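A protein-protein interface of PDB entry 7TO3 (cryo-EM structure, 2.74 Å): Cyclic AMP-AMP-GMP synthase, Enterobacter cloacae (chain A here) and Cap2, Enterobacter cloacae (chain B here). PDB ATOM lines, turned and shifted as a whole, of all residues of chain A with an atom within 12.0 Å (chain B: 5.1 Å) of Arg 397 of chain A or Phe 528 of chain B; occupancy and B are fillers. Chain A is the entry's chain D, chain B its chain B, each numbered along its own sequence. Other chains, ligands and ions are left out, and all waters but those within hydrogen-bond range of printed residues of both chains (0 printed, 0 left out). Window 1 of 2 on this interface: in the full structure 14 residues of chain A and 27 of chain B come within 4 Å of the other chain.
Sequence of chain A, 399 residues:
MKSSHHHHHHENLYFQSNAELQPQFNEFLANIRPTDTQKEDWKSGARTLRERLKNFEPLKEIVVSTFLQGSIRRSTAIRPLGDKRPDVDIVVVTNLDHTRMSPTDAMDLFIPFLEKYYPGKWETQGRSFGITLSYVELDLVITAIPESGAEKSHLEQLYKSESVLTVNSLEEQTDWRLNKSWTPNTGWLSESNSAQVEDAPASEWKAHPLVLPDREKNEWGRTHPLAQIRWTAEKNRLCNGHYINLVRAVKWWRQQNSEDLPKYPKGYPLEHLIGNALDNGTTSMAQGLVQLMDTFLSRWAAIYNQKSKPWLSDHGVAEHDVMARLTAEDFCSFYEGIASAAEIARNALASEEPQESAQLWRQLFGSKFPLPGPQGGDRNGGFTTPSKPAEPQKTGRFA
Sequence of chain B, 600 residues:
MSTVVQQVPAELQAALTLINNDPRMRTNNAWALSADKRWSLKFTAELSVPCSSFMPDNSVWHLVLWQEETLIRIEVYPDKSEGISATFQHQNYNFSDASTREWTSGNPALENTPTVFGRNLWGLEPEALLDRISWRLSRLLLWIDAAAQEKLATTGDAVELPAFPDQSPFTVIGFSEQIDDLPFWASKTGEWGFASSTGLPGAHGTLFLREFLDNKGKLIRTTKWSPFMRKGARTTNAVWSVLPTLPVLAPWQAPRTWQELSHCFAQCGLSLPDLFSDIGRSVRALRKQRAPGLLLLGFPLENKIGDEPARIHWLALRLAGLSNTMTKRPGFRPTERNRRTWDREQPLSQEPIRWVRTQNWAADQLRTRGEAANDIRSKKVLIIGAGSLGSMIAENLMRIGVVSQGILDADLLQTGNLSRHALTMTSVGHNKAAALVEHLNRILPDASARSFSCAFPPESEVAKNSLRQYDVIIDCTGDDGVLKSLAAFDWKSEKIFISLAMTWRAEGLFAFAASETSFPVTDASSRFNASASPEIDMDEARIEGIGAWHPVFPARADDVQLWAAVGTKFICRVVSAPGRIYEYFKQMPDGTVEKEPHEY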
ATOM      1  N   THR A  37      36.607  19.806  -1.720  1.00  0.00           N
ATOM      2  CA  THR A  37      37.053  18.426  -1.873  1.00  0.00           C
ATOM      3  C   THR A  37      38.378  18.217  -1.155  1.00  0.00           C
ATOM      4  O   THR A  37      38.535  17.275  -0.371  1.00  0.00           O
ATOM      5  CB  THR A  37      37.187  18.086  -3.364  1.00  0.00           C
ATOM      6  OG1 THR A  37      38.067  19.030  -3.989  1.00  0.00           O
ATOM      7  CG2 THR A  37      35.833  18.131  -4.068  1.00  0.00           C
ATOM      8  N   GLU A  40      37.720  18.256   2.845  1.00  0.00           N
ATOM      9  CA  GLU A  40      37.322  16.965   3.390  1.00  0.00           C
ATOM     10  C   GLU A  40      38.452  15.951   3.290  1.00  0.00           C
ATOM     11  O   GLU A  40      38.613  15.115   4.192  1.00  0.00           O
ATOM     12  CB  GLU A  40      36.058  16.465   2.686  1.00  0.00           C
ATOM     13  CG  GLU A  40      36.287  15.955   1.275  1.00  0.00           C
ATOM     14  CD  GLU A  40      35.147  15.105   0.748  1.00  0.00           C
ATOM     15  OE1 GLU A  40      34.194  14.821   1.507  1.00  0.00           O
ATOM     16  OE2 GLU A  40      35.185  14.747  -0.446  1.00  0.00           O
ATOM     17  N   TYR A 135      43.987  13.935  -2.964  1.00  0.00           N
ATOM     18  CA  TYR A 135      43.956  15.332  -3.377  1.00  0.00           C
ATOM     19  C   TYR A 135      44.919  16.236  -2.621  1.00  0.00           C
ATOM     20  O   TYR A 135      45.151  17.363  -3.075  1.00  0.00           O
ATOM     21  CB  TYR A 135      42.537  15.904  -3.232  1.00  0.00           C
ATOM     22  CG  TYR A 135      41.502  15.219  -4.097  1.00  0.00           C
ATOM     23  CD1 TYR A 135      41.492  15.395  -5.474  1.00  0.00           C
ATOM     24  CD2 TYR A 135      40.531  14.400  -3.535  1.00  0.00           C
ATOM     25  CE1 TYR A 135      40.546  14.772  -6.268  1.00  0.00           C
ATOM     26  CE2 TYR A 135      39.582  13.772  -4.320  1.00  0.00           C
ATOM     27  CZ  TYR A 135      39.594  13.961  -5.685  1.00  0.00           C
ATOM     28  OH  TYR A 135      38.652  13.339  -6.471  1.00  0.00           O
ATOM     29  N   GLN A 393      23.976  21.219  -9.414  1.00  0.00           N
ATOM     30  CA  GLN A 393      23.679  20.115 -10.320  1.00  0.00           C
ATOM     31  C   GLN A 393      23.780  18.773  -9.601  1.00  0.00           C
ATOM     32  O   GLN A 393      24.875  18.307  -9.286  1.00  0.00           O
ATOM     33  CB  GLN A 393      24.625  20.140 -11.523  1.00  0.00           C
ATOM     34  N   LYS A 394      22.630  18.156  -9.345  1.00  0.00           N
ATOM     35  CA  LYS A 394      22.555  16.870  -8.668  1.00  0.00           C
ATOM     36  C   LYS A 394      22.042  15.816  -9.638  1.00  0.00           C
ATOM     37  O   LYS A 394      21.000  16.006 -10.274  1.00  0.00           O
ATOM     38  CB  LYS A 394      21.645  16.950  -7.440  1.00  0.00           C
ATOM     39  N   THR A 395      22.773  14.710  -9.748  1.00  0.00           N
ATOM     40  CA  THR A 395      22.380  13.628 -10.636  1.00  0.00           C
ATOM     41  C   THR A 395      21.313  12.757  -9.984  1.00  0.00           C
ATOM     42  O   THR A 395      21.168  12.723  -8.758  1.00  0.00           O
ATOM     43  CB  THR A 395      23.591  12.773 -11.015  1.00  0.00           C
ATOM     44  OG1 THR A 395      23.200  11.786 -11.977  1.00  0.00           O
ATOM     45  CG2 THR A 395      24.166  12.081  -9.787  1.00  0.00           C
ATOM     46  N   GLY A 396      20.558  12.052 -10.822  1.00  0.00           N
ATOM     47  CA  GLY A 396      19.498  11.188 -10.338  1.00  0.00           C
ATOM     48  C   GLY A 396      19.956   9.772 -10.059  1.00  0.00           C
ATOM     49  O   GLY A 396      20.373   9.054 -10.973  1.00  0.00           O
ATOM     50  N   ARG A 397      19.882   9.359  -8.797  1.00  0.00           N
ATOM     51  CA  ARG A 397      20.252   8.015  -8.379  1.00  0.00           C
ATOM     52  C   ARG A 397      19.046   7.329  -7.754  1.00  0.00           C
ATOM     53  O   ARG A 397      18.334   7.925  -6.940  1.00  0.00           O
ATOM     54  CB  ARG A 397      21.418   8.044  -7.385  1.00  0.00           C
ATOM     55  CG  ARG A 397      22.634   8.811  -7.879  1.00  0.00           C
ATOM     56  CD  ARG A 397      23.729   8.851  -6.826  1.00  0.00           C
ATOM     57  NE  ARG A 397      23.254   9.411  -5.566  1.00  0.00           N
ATOM     58  CZ  ARG A 397      23.185   8.736  -4.426  1.00  0.00           C
ATOM     59  NH1 ARG A 397      23.556   7.469  -4.348  1.00  0.00           N
ATOM     60  NH2 ARG A 397      22.732   9.349  -3.336  1.00  0.00           N
ATOM     61  N   PHE A 398      18.822   6.074  -8.138  1.00  0.00           N
ATOM     62  CA  PHE A 398      17.662   5.321  -7.685  1.00  0.00           C
ATOM     63  C   PHE A 398      18.103   3.951  -7.195  1.00  0.00           C
ATOM     64  O   PHE A 398      19.094   3.398  -7.682  1.00  0.00           O
ATOM     65  CB  PHE A 398      16.625   5.171  -8.804  1.00  0.00           C
ATOM     66  CG  PHE A 398      16.325   6.452  -9.528  1.00  0.00           C
ATOM     67  CD1 PHE A 398      15.391   7.344  -9.027  1.00  0.00           C
ATOM     68  CD2 PHE A 398      16.981   6.767 -10.707  1.00  0.00           C
ATOM     69  CE1 PHE A 398      15.117   8.526  -9.691  1.00  0.00           C
ATOM     70  CE2 PHE A 398      16.710   7.946 -11.374  1.00  0.00           C
ATOM     71  CZ  PHE A 398      15.777   8.827 -10.866  1.00  0.00           C
ATOM     72  N   ALA A 399      17.363   3.408  -6.234  1.00  0.00           N
ATOM     73  CA  ALA A 399      17.668   2.095  -5.678  1.00  0.00           C
ATOM     74  C   ALA A 399      16.391   1.315  -5.381  1.00  0.00           C
ATOM     75  O   ALA A 399      16.295   0.098  -5.543  1.00  0.00           O
ATOM     76  CB  ALA A 399      18.510   2.233  -4.421  1.00  0.00           C
ATOM     77  N   GLY B 478      20.071   5.323  -2.469  1.00  0.00           N
ATOM     78  CA  GLY B 478      19.921   6.301  -3.526  1.00  0.00           C
ATOM     79  C   GLY B 478      19.478   7.667  -3.058  1.00  0.00           C
ATOM     80  O   GLY B 478      18.980   8.457  -3.865  1.00  0.00           O
ATOM     81  N   ASP B 479      19.647   7.971  -1.775  1.00  0.00           N
ATOM     82  CA  ASP B 479      19.220   9.234  -1.193  1.00  0.00           C
ATOM     83  C   ASP B 479      20.433  10.023  -0.716  1.00  0.00           C
ATOM     84  O   ASP B 479      21.361   9.458  -0.127  1.00  0.00           O
ATOM     85  CB  ASP B 479      18.253   8.998  -0.029  1.00  0.00           C
ATOM     86  CG  ASP B 479      17.653  10.285   0.501  1.00  0.00           C
ATOM     87  OD1 ASP B 479      17.466  11.229  -0.295  1.00  0.00           O
ATOM     88  OD2 ASP B 479      17.364  10.352   1.715  1.00  0.00           O
ATOM     89  N   ASP B 480      20.419  11.333  -0.974  1.00  0.00           N
ATOM     90  CA  ASP B 480      21.542  12.186  -0.601  1.00  0.00           C
ATOM     91  C   ASP B 480      21.570  12.485   0.893  1.00  0.00           C
ATOM     92  O   ASP B 480      22.654  12.659   1.469  1.00  0.00           O
ATOM     93  CB  ASP B 480      21.488  13.492  -1.397  1.00  0.00           C
ATOM     94  CG  ASP B 480      21.446  13.259  -2.895  1.00  0.00           C
ATOM     95  OD1 ASP B 480      21.722  12.120  -3.329  1.00  0.00           O
ATOM     96  OD2 ASP B 480      21.134  14.212  -3.639  1.00  0.00           O
ATOM     97  N   LEU B 483      23.586   9.997   2.571  1.00  0.00           N
ATOM     98  CA  LEU B 483      25.007  10.241   2.345  1.00  0.00           C
ATOM     99  C   LEU B 483      25.545  11.317   3.277  1.00  0.00           C
ATOM    100  O   LEU B 483      26.658  11.185   3.799  1.00  0.00           O
ATOM    101  CB  LEU B 483      25.251  10.630   0.886  1.00  0.00           C
ATOM    102  CG  LEU B 483      25.123   9.512  -0.152  1.00  0.00           C
ATOM    103  CD1 LEU B 483      25.780   9.918  -1.463  1.00  0.00           C
ATOM    104  CD2 LEU B 483      25.726   8.218   0.372  1.00  0.00           C
ATOM    105  N   SER B 499      29.017   2.449  -1.622  1.00  0.00           N
ATOM    106  CA  SER B 499      27.770   3.062  -2.062  1.00  0.00           C
ATOM    107  C   SER B 499      27.454   2.562  -3.464  1.00  0.00           C
ATOM    108  O   SER B 499      28.299   2.656  -4.365  1.00  0.00           O
ATOM    109  CB  SER B 499      27.870   4.588  -2.039  1.00  0.00           C
ATOM    110  OG  SER B 499      26.646   5.188  -2.421  1.00  0.00           O
ATOM    111  N   ALA B 501      24.397   2.521  -6.599  1.00  0.00           N
ATOM    112  CA  ALA B 501      23.143   3.112  -7.054  1.00  0.00           C
ATOM    113  C   ALA B 501      22.960   2.880  -8.547  1.00  0.00           C
ATOM    114  O   ALA B 501      23.928   2.667  -9.278  1.00  0.00           O
ATOM    115  CB  ALA B 501      23.083   4.612  -6.744  1.00  0.00           C
ATOM    116  N   MET B 502      21.709   2.928  -8.993  1.00  0.00           N
ATOM    117  CA  MET B 502      21.376   2.780 -10.403  1.00  0.00           C
ATOM    118  C   MET B 502      20.981   4.125 -11.005  1.00  0.00           C
ATOM    119  O   MET B 502      20.691   5.092 -10.297  1.00  0.00           O
ATOM    120  CB  MET B 502      20.244   1.766 -10.599  1.00  0.00           C
ATOM    121  CG  MET B 502      20.559   0.368 -10.095  1.00  0.00           C
ATOM    122  SD  MET B 502      19.215  -0.797 -10.396  1.00  0.00           S
ATOM    123  CE  MET B 502      17.901  -0.062  -9.428  1.00  0.00           C
ATOM    124  N   PHE B 510      26.391   3.192 -10.618  1.00  0.00           N
ATOM    125  CA  PHE B 510      27.478   3.852  -9.908  1.00  0.00           C
ATOM    126  C   PHE B 510      27.920   2.963  -8.754  1.00  0.00           C
ATOM    127  O   PHE B 510      27.083   2.537  -7.943  1.00  0.00           O
ATOM    128  CB  PHE B 510      27.043   5.208  -9.345  1.00  0.00           C
ATOM    129  CG  PHE B 510      26.332   6.091 -10.328  1.00  0.00           C
ATOM    130  CD1 PHE B 510      27.027   6.749 -11.327  1.00  0.00           C
ATOM    131  CD2 PHE B 510      24.964   6.290 -10.226  1.00  0.00           C
ATOM    132  CE1 PHE B 510      26.367   7.573 -12.220  1.00  0.00           C
ATOM    133  CE2 PHE B 510      24.301   7.112 -11.112  1.00  0.00           C
ATOM    134  CZ  PHE B 510      25.003   7.755 -12.113  1.00  0.00           C
ATOM    135  N   ALA B 511      29.228   2.701  -8.668  1.00  0.00           N
ATOM    136  CA  ALA B 511      29.809   1.974  -7.546  1.00  0.00           C
ATOM    137  C   ALA B 511      30.953   2.800  -6.976  1.00  0.00           C
ATOM    138  O   ALA B 511      31.868   3.185  -7.713  1.00  0.00           O
ATOM    139  CB  ALA B 511      30.307   0.592  -7.979  1.00  0.00           C
ATOM    140  N   PHE B 512      30.904   3.071  -5.671  1.00  0.00           N
ATOM    141  CA  PHE B 512      31.937   3.850  -5.001  1.00  0.00           C
ATOM    142  C   PHE B 512      32.351   3.136  -3.723  1.00  0.00           C
ATOM    143  O   PHE B 512      31.516   2.532  -3.046  1.00  0.00           O
ATOM    144  CB  PHE B 512      31.439   5.269  -4.685  1.00  0.00           C
ATOM    145  CG  PHE B 512      32.471   6.148  -4.036  1.00  0.00           C
ATOM    146  CD1 PHE B 512      33.444   6.774  -4.797  1.00  0.00           C
ATOM    147  CD2 PHE B 512      32.460   6.357  -2.666  1.00  0.00           C
ATOM    148  CE1 PHE B 512      34.392   7.588  -4.203  1.00  0.00           C
ATOM    149  CE2 PHE B 512      33.406   7.169  -2.067  1.00  0.00           C
ATOM    150  CZ  PHE B 512      34.372   7.785  -2.837  1.00  0.00           C
ATOM    151  N   ASP B 523      33.538  13.983  -2.654  1.00  0.00           N
ATOM    152  CA  ASP B 523      34.211  13.235  -3.712  1.00  0.00           C
ATOM    153  C   ASP B 523      33.245  12.289  -4.414  1.00  0.00           C
ATOM    154  O   ASP B 523      33.252  12.173  -5.646  1.00  0.00           O
ATOM    155  CB  ASP B 523      35.398  12.465  -3.131  1.00  0.00           C
ATOM    156  CG  ASP B 523      36.207  11.749  -4.194  1.00  0.00           C
ATOM    157  OD1 ASP B 523      36.251  12.239  -5.342  1.00  0.00           O
ATOM    158  OD2 ASP B 523      36.802  10.696  -3.880  1.00  0.00           O
ATOM    159  N   ALA B 524      32.401  11.604  -3.640  1.00  0.00           N
ATOM    160  CA  ALA B 524      31.429  10.687  -4.228  1.00  0.00           C
ATOM    161  C   ALA B 524      30.439  11.432  -5.115  1.00  0.00           C
ATOM    162  O   ALA B 524      30.110  10.976  -6.216  1.00  0.00           O
ATOM    163  CB  ALA B 524      30.698   9.919  -3.126  1.00  0.00           C
ATOM    164  N   SER B 525      29.955  12.587  -4.651  1.00  0.00           N
ATOM    165  CA  SER B 525      29.022  13.372  -5.453  1.00  0.00           C
ATOM    166  C   SER B 525      29.681  13.879  -6.731  1.00  0.00           C
ATOM    167  O   SER B 525      29.061  13.874  -7.803  1.00  0.00           O
ATOM    168  CB  SER B 525      28.473  14.537  -4.630  1.00  0.00           C
ATOM    169  OG  SER B 525      27.742  14.069  -3.511  1.00  0.00           O
ATOM    170  N   SER B 526      30.937  14.324  -6.636  1.00  0.00           N
ATOM    171  CA  SER B 526      31.651  14.780  -7.823  1.00  0.00           C
ATOM    172  C   SER B 526      31.826  13.649  -8.828  1.00  0.00           C
ATOM    173  O   SER B 526      31.650  13.848 -10.036  1.00  0.00           O
ATOM    174  CB  SER B 526      33.007  15.365  -7.427  1.00  0.00           C
ATOM    175  OG  SER B 526      33.779  15.684  -8.572  1.00  0.00           O
ATOM    176  N   ARG B 527      32.173  12.452  -8.348  1.00  0.00           N
ATOM    177  CA  ARG B 527      32.317  11.313  -9.248  1.00  0.00           C
ATOM    178  C   ARG B 527      30.983  10.929  -9.878  1.00  0.00           C
ATOM    179  O   ARG B 527      30.931  10.571 -11.061  1.00  0.00           O
ATOM    180  CB  ARG B 527      32.927  10.124  -8.505  1.00  0.00           C
ATOM    181  CG  ARG B 527      34.359  10.346  -8.023  1.00  0.00           C
ATOM    182  CD  ARG B 527      35.374  10.298  -9.165  1.00  0.00           C
ATOM    183  NE  ARG B 527      35.393  11.522  -9.959  1.00  0.00           N
ATOM    184  CZ  ARG B 527      36.046  12.626  -9.621  1.00  0.00           C
ATOM    185  NH1 ARG B 527      36.749  12.698  -8.503  1.00  0.00           N
ATOM    186  NH2 ARG B 527      35.992  13.684 -10.426  1.00  0.00           N
ATOM    187  N   PHE B 528      29.894  10.991  -9.105  1.00  0.00           N
ATOM    188  CA  PHE B 528      28.579  10.689  -9.660  1.00  0.00           C
ATOM    189  C   PHE B 528      28.195  11.686 -10.746  1.00  0.00           C
ATOM    190  O   PHE B 528      27.649  11.303 -11.787  1.00  0.00           O
ATOM    191  CB  PHE B 528      27.524  10.678  -8.553  1.00  0.00           C
ATOM    192  CG  PHE B 528      27.723   9.597  -7.530  1.00  0.00           C
ATOM    193  CD1 PHE B 528      28.368   8.418  -7.861  1.00  0.00           C
ATOM    194  CD2 PHE B 528      27.252   9.758  -6.235  1.00  0.00           C
ATOM    195  CE1 PHE B 528      28.549   7.421  -6.919  1.00  0.00           C
ATOM    196  CE2 PHE B 528      27.430   8.766  -5.290  1.00  0.00           C
ATOM    197  CZ  PHE B 528      28.079   7.596  -5.632  1.00  0.00           C
ATOM    198  N   ASN B 529      28.472  12.972 -10.520  1.00  0.00           N
ATOM    199  CA  ASN B 529      28.107  13.990 -11.501  1.00  0.00           C
ATOM    200  C   ASN B 529      28.992  13.930 -12.742  1.00  0.00           C
ATOM    201  O   ASN B 529      28.525  14.211 -13.852  1.00  0.00           O
ATOM    202  CB  ASN B 529      28.176  15.380 -10.867  1.00  0.00           C
ATOM    203  CG  ASN B 529      27.174  15.557  -9.743  1.00  0.00           C
ATOM    204  OD1 ASN B 529      26.249  14.760  -9.588  1.00  0.00           O
ATOM    205  ND2 ASN B 529      27.353  16.608  -8.952  1.00  0.00           N
ATOM    206  N   ALA B 530      30.267  13.571 -12.576  1.00  0.00           N
ATOM    207  CA  ALA B 530      31.188  13.570 -13.709  1.00  0.00           C
ATOM    208  C   ALA B 530      30.859  12.471 -14.713  1.00  0.00           C
ATOM    209  O   ALA B 530      31.108  12.635 -15.912  1.00  0.00           O
ATOM    210  CB  ALA B 530      32.628  13.423 -13.216  1.00  0.00           C
ATOM    211  N   SER B 531      30.313  11.350 -14.247  1.00  0.00           N
ATOM    212  CA  SER B 531      30.026  10.232 -15.135  1.00  0.00           C
ATOM    213  C   SER B 531      28.921  10.592 -16.122  1.00  0.00           C
ATOM    214  O   SER B 531      28.011  11.364 -15.810  1.00  0.00           O
ATOM    215  CB  SER B 531      29.624   9.001 -14.323  1.00  0.00           C
ATOM    216  OG  SER B 531      30.760   8.381 -13.744  1.00  0.00           O
ATOM    217  N   TYR B 582      36.277   3.980  -7.637  1.00  0.00           N
ATOM    218  CA  TYR B 582      35.016   4.368  -8.260  1.00  0.00           C
ATOM    219  C   TYR B 582      34.916   3.724  -9.632  1.00  0.00           C
ATOM    220  O   TYR B 582      35.884   3.737 -10.398  1.00  0.00           O
ATOM    221  CB  TYR B 582      34.887   5.888  -8.390  1.00  0.00           C
ATOM    222  CG  TYR B 582      33.627   6.305  -9.113  1.00  0.00           C
ATOM    223  CD1 TYR B 582      32.388   6.216  -8.494  1.00  0.00           C
ATOM    224  CD2 TYR B 582      33.675   6.770 -10.421  1.00  0.00           C
ATOM    225  CE1 TYR B 582      31.232   6.587  -9.153  1.00  0.00           C
ATOM    226  CE2 TYR B 582      32.524   7.143 -11.088  1.00  0.00           C
ATOM    227  CZ  TYR B 582      31.306   7.050 -10.449  1.00  0.00           C
ATOM    228  OH  TYR B 582      30.157   7.421 -11.109  1.00  0.00           O
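The backbone carbonyl oxygen of Arg 527 of chain B is in hydrogen-bond range of the side-chain hydroxyl of Tyr 582 of chain B (3.2 Å). The side-chain amide nitrogen of Asn 529 of chain B sits close to the backbone carbonyl oxygen of Ser 525 of chain B (3.4 Å). The backbone NH of Phe 510 of chain B is in hydrogen-bond range of the backbone carbonyl oxygen of Ala 501 of chain B, 2.9 Å away. O of Arg 527 of chain B sits at hydrogen-bond distance from OG of Ser 531 of chain B. The guanidinium group (NH1) of Arg 527 of chain B lies within salt-bridge range of the side-chain carboxylate (OD1) of Asp 523 of chain B (3.2 Å).
The side-chain carboxylate of Asp 480 of chain B is in salt-bridge range of the guanidinium group of Arg 397 of chain A, at 2.9 Å. The guanidinium group (NH1) of Arg 527 of chain B lies within hydrogen-bond range of the side-chain hydroxyl (OH) of Tyr 135 of chain A (2.9 Å). The backbone carbonyl oxygen of Asp 479 of chain B is in hydrogen-bond range of the guanidinium group of Arg 397 of chain A, 3.5 Å away. O of Phe 398 of chain A sits at hydrogen-bond distance from N of Met 502 of chain B (3.0 Å). ND2 of Asn 529 of chain B sits at hydrogen-bond distance from O of Gln 393 of chain A (3.0 Å). The side-chain hydroxyl (OH) of Tyr 135 of chain A is in hydrogen-bond range of the side-chain carboxylate (OD1) of Asp 523 of chain B, at 2.9 Å. OD1 of Asn 529 of chain B lies close to N of Thr 395 of chain A (3.5 Å). The backbone carbonyl oxygen (O) of Arg 397 of chain A sits close to the backbone carbonyl oxygen (O) of Gly 478 of chain B. OE2 of Glu 40 of chain A sits at hydrogen-bond distance from N of Asp 523 of chain B (2.9 Å).
Hydrophobic or aromatic side chains of chain B that line the printed part of chain A: Leu 483, Ala 501, Met 502 and Phe 528. Hydrophobic or aromatic side chains of chain A within 4 Å of the printed part of chain B: Tyr 135 and Ala 399. Among the printed residues, Asp or Glu carboxylates within 4 Å of a Lys or Arg side-chain nitrogen of the other chain: Arg 397 of chain A with Asp 480 of chain B (2.9 Å).
Printed residues of chain B within 4 Å of Arg 397 of chain A: Gly 478 (3.2 Å), Asp 479 (3.5 Å), Asp 480 (2.9 Å), Leu 483 (3.6 Å), Ala 501 (3.8 Å), Met 502 (3.5 Å) and Phe 528 (3.7 Å). Phe 528 of chain B touches two residues of chain A. Asp 480 of chain B touches just one residue of chain A: Arg 397 (2.9 Å). No residue of chain A comes within 4 Å of Ser 499 of chain B. No residue of chain A comes within 4 Å of Phe 512 of chain B. No residue of chain A comes within 4 Å of Ala 524 of chain B. Ser 526 of chain B touches none of the printed residues of chain A. Arg 527 of chain B touches just one residue of chain A: Tyr 135. Asn 529 of chain B touches just these residues of chain A: Gln 393 (3.0 Å) and Thr 395 (3.4 Å). No residue of chain A comes within 4 Å of Ser 531 of chain B. Of the printed residues of chain B, Phe 398 of chain A touches Ala 501 (3.995 Å) and Met 502 (3.0 Å). Printed residues of chain B within 4 Å of Gln 393 of chain A: Asn 529 (3.0 Å). Gly 396 of chain A touches none of the printed residues of chain B. Lys 394 of chain A touches none of the printed residues of chain B. The nearest printed residue of chain B that does not touch Arg 397 of chain A is Phe 510 of chain B (4.01 Å).
CG2 of Thr 395 of chain A touches CB of Phe 528 of chain B (3.8 Å). Arg 397 of chain A touches Leu 483 of chain B (NH2 to CD1, 3.6 Å). Arg 397 of chain A touches Ala 501 of chain B (NH1 to CB, 3.8 Å). Arg 397 of chain A touches Met 502 of chain B (CA to O, 3.5 Å). CD of Arg 397 of chain A touches CD2 of Phe 528 of chain B, 3.7 Å away. Phe 398 of chain A touches Ala 501 of chain B (O to C, 3.995 Å). N of Gly 478 of chain B touches CB of Ala 399 of chain A, 3.97 Å away.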
